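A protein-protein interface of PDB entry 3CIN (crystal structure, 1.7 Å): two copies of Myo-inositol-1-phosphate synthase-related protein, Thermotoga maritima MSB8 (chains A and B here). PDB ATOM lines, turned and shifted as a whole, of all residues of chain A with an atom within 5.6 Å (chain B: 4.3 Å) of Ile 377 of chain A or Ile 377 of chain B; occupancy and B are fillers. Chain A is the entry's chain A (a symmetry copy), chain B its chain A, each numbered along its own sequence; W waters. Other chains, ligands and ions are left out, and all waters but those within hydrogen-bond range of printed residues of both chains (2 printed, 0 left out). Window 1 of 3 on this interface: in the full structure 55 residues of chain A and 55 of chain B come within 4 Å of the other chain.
OE1 of Gln 238 of chain B touches O of Arg 376 of chain A (3.6 Å). CD1 of Ile 377 of chain A touches CB of Ser 234 of chain B, 3.9 Å away. Ile 377 of chain A touches Gln 238 of chain B. Ile 378 of chain B touches Ile 377 of chain A. CG1 of Ile 378 of chain A touches CG2 of Ile 377 of chain B, 3.95 Å away. Glu 381 of chain B touches Ile 378 of chain A (OE2 to CD1, 3.6 Å). Glu 381 of chain A touches Ile 378 of chain B. Trp 393 of chain A touches Ser 234 of chain B. NE2 of Gln 238 of chain B touches CZ3 of Trp 393 of chain A, at 3.8 Å. Trp 393 of chain A touches Pro 375 of chain B.
OE2 of Glu 381 of chain A is in hydrogen-bond range of N of Trp 393 of chain A.
Water W2 bridges the backbone carbonyl oxygen (O) of Gln 238 of chain B (2.6 Å) and the side-chain hydroxyl (OH) of Tyr 380 of chain A (2.6 Å). Water W1 lies within hydrogen-bond range of O of Gln 238 of chain A (2.6 Å) and OH of Tyr 380 of chain B (2.6 Å).
Gln 238 of chain A touches Arg 376 of chain B, and with the chains exchanged Arg 376 of chain A touches Gln 238 of chain B. Gln 238 of chain A touches Ile 377 of chain B, and with the chains exchanged Ile 377 of chain A touches Gln 238 of chain B. Gln 238 of chain A touches Tyr 380 of chain B, and with the chains exchanged Tyr 380 of chain A touches Gln 238 of chain B. Ile 377 of chain B touches its own counterpart, Ile 377 of chain A.
Of the printed residues of chain B, Ile 377 of chain A touches Ser 234 (3.9 Å), Gln 238 (3.0 Å), Ile 377 (3.99 Å) and Ile 378 (3.95 Å). Of the printed residues of chain A, Ile 377 of chain B touches Ser 234 (3.9 Å), Gln 238 (3.0 Å), Ile 377 (3.99 Å) and Ile 378 (3.95 Å). Printed residues of chain B within 4 Å of Trp 393 of chain A: Ser 234 (3.9 Å), Gln 238 (3.8 Å), Pro 375 (3.4 Å) and Ile 378 (3.7 Å). Printed residues of chain A within 4 Å of Tyr 380 of chain B: Gln 238 (3.1 Å). Ala 379 of chain A touches none of the printed residues of chain B. The nearest printed residue of chain B that does not touch Glu 381 of chain A is Gln 238 of chain B (5.2 Å).
Printed residues of chain B that touch a printed residue of chain A: Ser 234, Gln 238, Pro 375, Arg 376, Ile 377, Ile 378, Tyr 380 and Glu 381. Hydrophobic or aromatic side chains of chain B that line the printed part of chain A: Pro 375, Ile 377, Ile 378 and Tyr 380. Hydrophobic or aromatic side chains of chain A within 4 Å of the printed part of chain B: Ile 377, Ile 378, Tyr 380 and Trp 393. Among the printed residues, no Asp or Glu carboxylate lies within 4 Å of a Lys or Arg side-chain nitrogen of the other chain.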
ATOM      1  N   ASP A 231     -14.698 -14.127  30.156  1.00  0.00           N
ATOM      2  CA  ASP A 231     -15.439 -15.269  30.667  1.00  0.00           C
ATOM      3  C   ASP A 231     -16.862 -14.881  31.087  1.00  0.00           C
ATOM      4  O   ASP A 231     -17.847 -15.560  30.738  1.00  0.00           O
ATOM      5  CB  ASP A 231     -14.741 -15.813  31.880  1.00  0.00           C
ATOM      6  CG  ASP A 231     -13.300 -16.211  31.637  1.00  0.00           C
ATOM      7  OD1 ASP A 231     -12.914 -16.569  30.491  1.00  0.00           O
ATOM      8  OD2 ASP A 231     -12.546 -16.214  32.648  1.00  0.00           O
ATOM      9  N   SER A 234     -18.935 -14.169  28.018  1.00  0.00           N
ATOM     10  CA  SER A 234     -19.304 -15.388  27.313  1.00  0.00           C
ATOM     11  C   SER A 234     -20.567 -15.989  27.937  1.00  0.00           C
ATOM     12  O   SER A 234     -21.479 -16.385  27.215  1.00  0.00           O
ATOM     13  CB  SER A 234     -18.161 -16.397  27.291  1.00  0.00           C
ATOM     14  OG  SER A 234     -17.045 -15.897  26.521  1.00  0.00           O
ATOM     15  N   HIS A 235     -20.612 -16.066  29.263  1.00  0.00           N
ATOM     16  CA  HIS A 235     -21.772 -16.503  30.098  1.00  0.00           C
ATOM     17  C   HIS A 235     -23.020 -15.721  29.742  1.00  0.00           C
ATOM     18  O   HIS A 235     -24.119 -16.233  29.527  1.00  0.00           O
ATOM     19  CB  HIS A 235     -21.433 -16.231  31.606  1.00  0.00           C
ATOM     20  CG  HIS A 235     -22.290 -16.981  32.596  1.00  0.00           C
ATOM     21  ND1 HIS A 235     -23.209 -16.367  33.424  1.00  0.00           N
ATOM     22  CD2 HIS A 235     -22.342 -18.300  32.899  1.00  0.00           C
ATOM     23  CE1 HIS A 235     -23.794 -17.279  34.188  1.00  0.00           C
ATOM     24  NE2 HIS A 235     -23.287 -18.459  33.884  1.00  0.00           N
ATOM     25  N   GLN A 238     -24.418 -16.336  26.100  1.00  0.00           N
ATOM     26  CA  GLN A 238     -25.165 -17.605  26.066  1.00  0.00           C
ATOM     27  C   GLN A 238     -26.612 -17.526  26.475  1.00  0.00           C
ATOM     28  O   GLN A 238     -27.470 -18.198  25.898  1.00  0.00           O
ATOM     29  CB  GLN A 238     -24.500 -18.621  27.009  1.00  0.00           C
ATOM     30  CG  GLN A 238     -23.291 -19.079  26.466  1.00  0.00           C
ATOM     31  CD  GLN A 238     -22.828 -20.336  27.051  1.00  0.00           C
ATOM     32  OE1 GLN A 238     -23.030 -20.649  28.272  1.00  0.00           O
ATOM     33  NE2 GLN A 238     -22.140 -21.088  26.210  1.00  0.00           N
ATOM     34  N   PRO A 375     -14.795 -17.573  23.113  1.00  0.00           N
ATOM     35  CA  PRO A 375     -14.792 -18.050  24.492  1.00  0.00           C
ATOM     36  C   PRO A 375     -13.636 -19.010  24.778  1.00  0.00           C
ATOM     37  O   PRO A 375     -13.389 -19.920  24.031  1.00  0.00           O
ATOM     38  CB  PRO A 375     -16.131 -18.756  24.620  1.00  0.00           C
ATOM     39  CG  PRO A 375     -16.983 -17.931  23.741  1.00  0.00           C
ATOM     40  CD  PRO A 375     -16.127 -17.725  22.530  1.00  0.00           C
ATOM     41  N   ARG A 376     -12.946 -18.768  25.881  1.00  0.00           N
ATOM     42  CA  ARG A 376     -11.704 -19.472  26.130  1.00  0.00           C
ATOM     43  C   ARG A 376     -11.851 -20.966  26.444  1.00  0.00           C
ATOM     44  O   ARG A 376     -10.914 -21.726  26.208  1.00  0.00           O
ATOM     45  CB  ARG A 376     -10.894 -18.759  27.210  1.00  0.00           C
ATOM     46  CG  ARG A 376      -9.440 -18.612  26.823  1.00  0.00           C
ATOM     47  CD  ARG A 376      -8.701 -17.438  27.597  1.00  0.00           C
ATOM     48  NE  ARG A 376      -8.894 -16.111  27.027  1.00  0.00           N
ATOM     49  CZ  ARG A 376      -8.238 -15.642  25.973  1.00  0.00           C
ATOM     50  NH1 ARG A 376      -7.336 -16.388  25.378  1.00  0.00           N
ATOM     51  NH2 ARG A 376      -8.488 -14.422  25.515  1.00  0.00           N
ATOM     52  N   ILE A 377     -13.018 -21.413  26.908  1.00  0.00           N
ATOM     53  CA  ILE A 377     -13.267 -22.853  27.068  1.00  0.00           C
ATOM     54  C   ILE A 377     -13.310 -23.548  25.720  1.00  0.00           C
ATOM     55  O   ILE A 377     -12.810 -24.673  25.549  1.00  0.00           O
ATOM     56  CB  ILE A 377     -14.546 -23.117  27.974  1.00  0.00           C
ATOM     57  CG1 ILE A 377     -14.250 -22.628  29.415  1.00  0.00           C
ATOM     58  CG2 ILE A 377     -14.851 -24.630  28.101  1.00  0.00           C
ATOM     59  CD1 ILE A 377     -15.448 -22.259  30.316  1.00  0.00           C
ATOM     60  N   ILE A 378     -13.937 -22.896  24.733  1.00  0.00           N
ATOM     61  CA  ILE A 378     -13.921 -23.406  23.360  1.00  0.00           C
ATOM     62  C   ILE A 378     -12.487 -23.409  22.789  1.00  0.00           C
ATOM     63  O   ILE A 378     -12.033 -24.420  22.223  1.00  0.00           O
ATOM     64  CB  ILE A 378     -14.888 -22.609  22.488  1.00  0.00           C
ATOM     65  CG1 ILE A 378     -16.311 -22.735  23.037  1.00  0.00           C
ATOM     66  CG2 ILE A 378     -14.846 -23.087  21.040  1.00  0.00           C
ATOM     67  CD1 ILE A 378     -17.316 -21.841  22.243  1.00  0.00           C
ATOM     68  N   ALA A 379     -11.772 -22.304  22.975  1.00  0.00           N
ATOM     69  CA  ALA A 379     -10.368 -22.235  22.582  1.00  0.00           C
ATOM     70  C   ALA A 379      -9.549 -23.353  23.235  1.00  0.00           C
ATOM     71  O   ALA A 379      -8.727 -23.974  22.571  1.00  0.00           O
ATOM     72  CB  ALA A 379      -9.754 -20.916  22.883  1.00  0.00           C
ATOM     73  N   TYR A 380      -9.772 -23.599  24.513  1.00  0.00           N
ATOM     74  CA  TYR A 380      -9.068 -24.665  25.235  1.00  0.00           C
ATOM     75  C   TYR A 380      -9.288 -26.018  24.610  1.00  0.00           C
ATOM     76  O   TYR A 380      -8.335 -26.784  24.359  1.00  0.00           O
ATOM     77  CB  TYR A 380      -9.527 -24.653  26.708  1.00  0.00           C
ATOM     78  CG  TYR A 380      -8.883 -25.736  27.546  1.00  0.00           C
ATOM     79  CD1 TYR A 380      -7.566 -25.619  27.975  1.00  0.00           C
ATOM     80  CD2 TYR A 380      -9.604 -26.855  27.899  1.00  0.00           C
ATOM     81  CE1 TYR A 380      -6.983 -26.633  28.746  1.00  0.00           C
ATOM     82  CE2 TYR A 380      -9.067 -27.822  28.669  1.00  0.00           C
ATOM     83  CZ  TYR A 380      -7.752 -27.723  29.096  1.00  0.00           C
ATOM     84  OH  TYR A 380      -7.228 -28.772  29.843  1.00  0.00           O
ATOM     85  N   GLU A 381     -10.545 -26.372  24.304  1.00  0.00           N
ATOM     86  CA  GLU A 381     -10.774 -27.703  23.757  1.00  0.00           C
ATOM     87  C   GLU A 381     -10.141 -27.827  22.379  1.00  0.00           C
ATOM     88  O   GLU A 381      -9.532 -28.854  22.055  1.00  0.00           O
ATOM     89  CB  GLU A 381     -12.255 -28.041  23.719  1.00  0.00           C
ATOM     90  CG  GLU A 381     -12.875 -28.089  25.141  1.00  0.00           C
ATOM     91  CD  GLU A 381     -12.610 -29.404  25.967  1.00  0.00           C
ATOM     92  OE1 GLU A 381     -11.465 -29.983  26.060  1.00  0.00           O
ATOM     93  OE2 GLU A 381     -13.621 -29.868  26.562  1.00  0.00           O
ATOM     94  N   LYS A 382     -10.223 -26.773  21.577  1.00  0.00           N
ATOM     95  CA  LYS A 382      -9.574 -26.805  20.249  1.00  0.00           C
ATOM     96  C   LYS A 382      -8.045 -26.843  20.290  1.00  0.00           C
ATOM     97  O   LYS A 382      -7.417 -27.464  19.449  1.00  0.00           O
ATOM     98  CB  LYS A 382     -10.048 -25.623  19.414  1.00  0.00           C
ATOM     99  CG  LYS A 382     -11.535 -25.721  19.041  1.00  0.00           C
ATOM    100  CD  LYS A 382     -11.963 -24.525  18.170  1.00  0.00           C
ATOM    101  CE  LYS A 382     -13.413 -24.643  17.639  1.00  0.00           C
ATOM    102  NZ  LYS A 382     -13.526 -25.172  16.230  1.00  0.00           N
ATOM    103  N   TRP A 393     -13.592 -32.375  28.934  1.00  0.00           N
ATOM    104  CA  TRP A 393     -14.914 -32.713  29.454  1.00  0.00           C
ATOM    105  C   TRP A 393     -15.722 -33.500  28.409  1.00  0.00           C
ATOM    106  O   TRP A 393     -16.318 -32.915  27.492  1.00  0.00           O
ATOM    107  CB  TRP A 393     -15.642 -31.429  29.869  1.00  0.00           C
ATOM    108  CG  TRP A 393     -15.096 -30.719  31.106  1.00  0.00           C
ATOM    109  CD1 TRP A 393     -15.365 -31.020  32.401  1.00  0.00           C
ATOM    110  CD2 TRP A 393     -14.251 -29.542  31.136  1.00  0.00           C
ATOM    111  NE1 TRP A 393     -14.747 -30.109  33.251  1.00  0.00           N
ATOM    112  CE2 TRP A 393     -14.068 -29.190  32.498  1.00  0.00           C
ATOM    113  CE3 TRP A 393     -13.649 -28.755  30.148  1.00  0.00           C
ATOM    114  CZ2 TRP A 393     -13.287 -28.117  32.892  1.00  0.00           C
ATOM    115  CZ3 TRP A 393     -12.890 -27.679  30.534  1.00  0.00           C
ATOM    116  CH2 TRP A 393     -12.727 -27.358  31.902  1.00  0.00           C
ATOM    117  N   SER B 234     -14.708 -23.481  36.160  1.00  0.00           N
ATOM    118  CA  SER B 234     -14.374 -24.036  34.857  1.00  0.00           C
ATOM    119  C   SER B 234     -13.109 -23.363  34.313  1.00  0.00           C
ATOM    120  O   SER B 234     -12.218 -24.045  33.813  1.00  0.00           O
ATOM    121  CB  SER B 234     -15.534 -23.911  33.875  1.00  0.00           C
ATOM    122  OG  SER B 234     -16.656 -24.719  34.297  1.00  0.00           O
ATOM    123  N   GLN B 238      -9.302 -25.209  33.666  1.00  0.00           N
ATOM    124  CA  GLN B 238      -8.577 -25.096  32.388  1.00  0.00           C
ATOM    125  C   GLN B 238      -7.121 -24.725  32.489  1.00  0.00           C
ATOM    126  O   GLN B 238      -6.286 -25.228  31.734  1.00  0.00           O
ATOM    127  CB  GLN B 238      -9.241 -24.023  31.510  1.00  0.00           C
ATOM    128  CG  GLN B 238     -10.468 -24.483  31.012  1.00  0.00           C
ATOM    129  CD  GLN B 238     -10.941 -23.738  29.847  1.00  0.00           C
ATOM    130  OE1 GLN B 238     -10.721 -22.491  29.685  1.00  0.00           O
ATOM    131  NE2 GLN B 238     -11.658 -24.467  29.010  1.00  0.00           N
ATOM    132  N   PRO B 375     -19.001 -27.852  32.253  1.00  0.00           N
ATOM    133  CA  PRO B 375     -18.985 -26.424  31.952  1.00  0.00           C
ATOM    134  C   PRO B 375     -20.151 -26.001  31.058  1.00  0.00           C
ATOM    135  O   PRO B 375     -20.429 -26.624  30.067  1.00  0.00           O
ATOM    136  CB  PRO B 375     -17.655 -26.232  31.242  1.00  0.00           C
ATOM    137  CG  PRO B 375     -16.807 -27.222  31.934  1.00  0.00           C
ATOM    138  CD  PRO B 375     -17.683 -28.434  32.005  1.00  0.00           C
ATOM    139  N   ARG B 376     -20.815 -24.925  31.449  1.00  0.00           N
ATOM    140  CA  ARG B 376     -22.064 -24.569  30.806  1.00  0.00           C
ATOM    141  C   ARG B 376     -21.937 -24.074  29.359  1.00  0.00           C
ATOM    142  O   ARG B 376     -22.891 -24.196  28.594  1.00  0.00           O
ATOM    143  CB  ARG B 376     -22.841 -23.573  31.663  1.00  0.00           C
ATOM    144  CG  ARG B 376     -24.300 -23.950  31.789  1.00  0.00           C
ATOM    145  CD  ARG B 376     -25.003 -23.316  33.065  1.00  0.00           C
ATOM    146  NE  ARG B 376     -24.798 -24.051  34.306  1.00  0.00           N
ATOM    147  CZ  ARG B 376     -25.467 -25.143  34.653  1.00  0.00           C
ATOM    148  NH1 ARG B 376     -26.393 -25.625  33.856  1.00  0.00           N
ATOM    149  NH2 ARG B 376     -25.204 -25.754  35.801  1.00  0.00           N
ATOM    150  N   ILE B 377     -20.769 -23.578  28.951  1.00  0.00           N
ATOM    151  CA  ILE B 377     -20.542 -23.243  27.538  1.00  0.00           C
ATOM    152  C   ILE B 377     -20.536 -24.494  26.680  1.00  0.00           C
ATOM    153  O   ILE B 377     -21.060 -24.515  25.553  1.00  0.00           O
ATOM    154  CB  ILE B 377     -19.250 -22.333  27.364  1.00  0.00           C
ATOM    155  CG1 ILE B 377     -19.510 -20.960  28.035  1.00  0.00           C
ATOM    156  CG2 ILE B 377     -18.968 -22.024  25.873  1.00  0.00           C
ATOM    157  CD1 ILE B 377     -18.288 -20.132  28.489  1.00  0.00           C
ATOM    158  N   ILE B 378     -19.918 -25.566  27.191  1.00  0.00           N
ATOM    159  CA  ILE B 378     -19.970 -26.863  26.515  1.00  0.00           C
ATOM    160  C   ILE B 378     -21.414 -27.405  26.468  1.00  0.00           C
ATOM    161  O   ILE B 378     -21.897 -27.833  25.404  1.00  0.00           O
ATOM    162  CB  ILE B 378     -19.006 -27.845  27.178  1.00  0.00           C
ATOM    163  CG1 ILE B 378     -17.575 -27.309  27.093  1.00  0.00           C
ATOM    164  CG2 ILE B 378     -19.084 -29.221  26.525  1.00  0.00           C
ATOM    165  CD1 ILE B 378     -16.570 -28.225  27.863  1.00  0.00           C
ATOM    166  N   ALA B 379     -22.107 -27.347  27.602  1.00  0.00           N
ATOM    167  CA  ALA B 379     -23.516 -27.721  27.648  1.00  0.00           C
ATOM    168  C   ALA B 379     -24.341 -26.919  26.637  1.00  0.00           C
ATOM    169  O   ALA B 379     -25.187 -27.486  25.954  1.00  0.00           O
ATOM    170  CB  ALA B 379     -24.102 -27.577  29.006  1.00  0.00           C
ATOM    171  N   TYR B 380     -24.098 -25.625  26.548  1.00  0.00           N
ATOM    172  CA  TYR B 380     -24.806 -24.763  25.594  1.00  0.00           C
ATOM    173  C   TYR B 380     -24.621 -25.218  24.170  1.00  0.00           C
ATOM    174  O   TYR B 380     -25.592 -25.355  23.397  1.00  0.00           O
ATOM    175  CB  TYR B 380     -24.318 -23.312  25.780  1.00  0.00           C
ATOM    176  CG  TYR B 380     -24.964 -22.334  24.823  1.00  0.00           C
ATOM    177  CD1 TYR B 380     -26.270 -21.900  25.018  1.00  0.00           C
ATOM    178  CD2 TYR B 380     -24.256 -21.857  23.743  1.00  0.00           C
ATOM    179  CE1 TYR B 380     -26.856 -20.998  24.119  1.00  0.00           C
ATOM    180  CE2 TYR B 380     -24.794 -20.963  22.889  1.00  0.00           C
ATOM    181  CZ  TYR B 380     -26.099 -20.529  23.067  1.00  0.00           C
ATOM    182  OH  TYR B 380     -26.626 -19.648  22.129  1.00  0.00           O
ATOM    183  N   GLU B 381     -23.377 -25.499  23.756  1.00  0.00           N
ATOM    184  CA  GLU B 381     -23.181 -25.879  22.363  1.00  0.00           C
ATOM    185  C   GLU B 381     -23.843 -27.220  22.080  1.00  0.00           C
ATOM    186  O   GLU B 381     -24.476 -27.403  21.033  1.00  0.00           O
ATOM    187  CB  GLU B 381     -21.707 -25.900  21.994  1.00  0.00           C
ATOM    188  CG  GLU B 381     -21.060 -24.494  22.111  1.00  0.00           C
ATOM    189  CD  GLU B 381     -21.332 -23.507  20.915  1.00  0.00           C
ATOM    190  OE1 GLU B 381     -22.485 -23.323  20.374  1.00  0.00           O
ATOM    191  OE2 GLU B 381     -20.318 -22.876  20.509  1.00  0.00           O
HETATM  192  O   HOH W   1     -27.986 -17.864  23.406  1.00  0.00           O
HETATM  193  O   HOH W   2      -5.813 -27.751  31.745  1.00  0.00           O
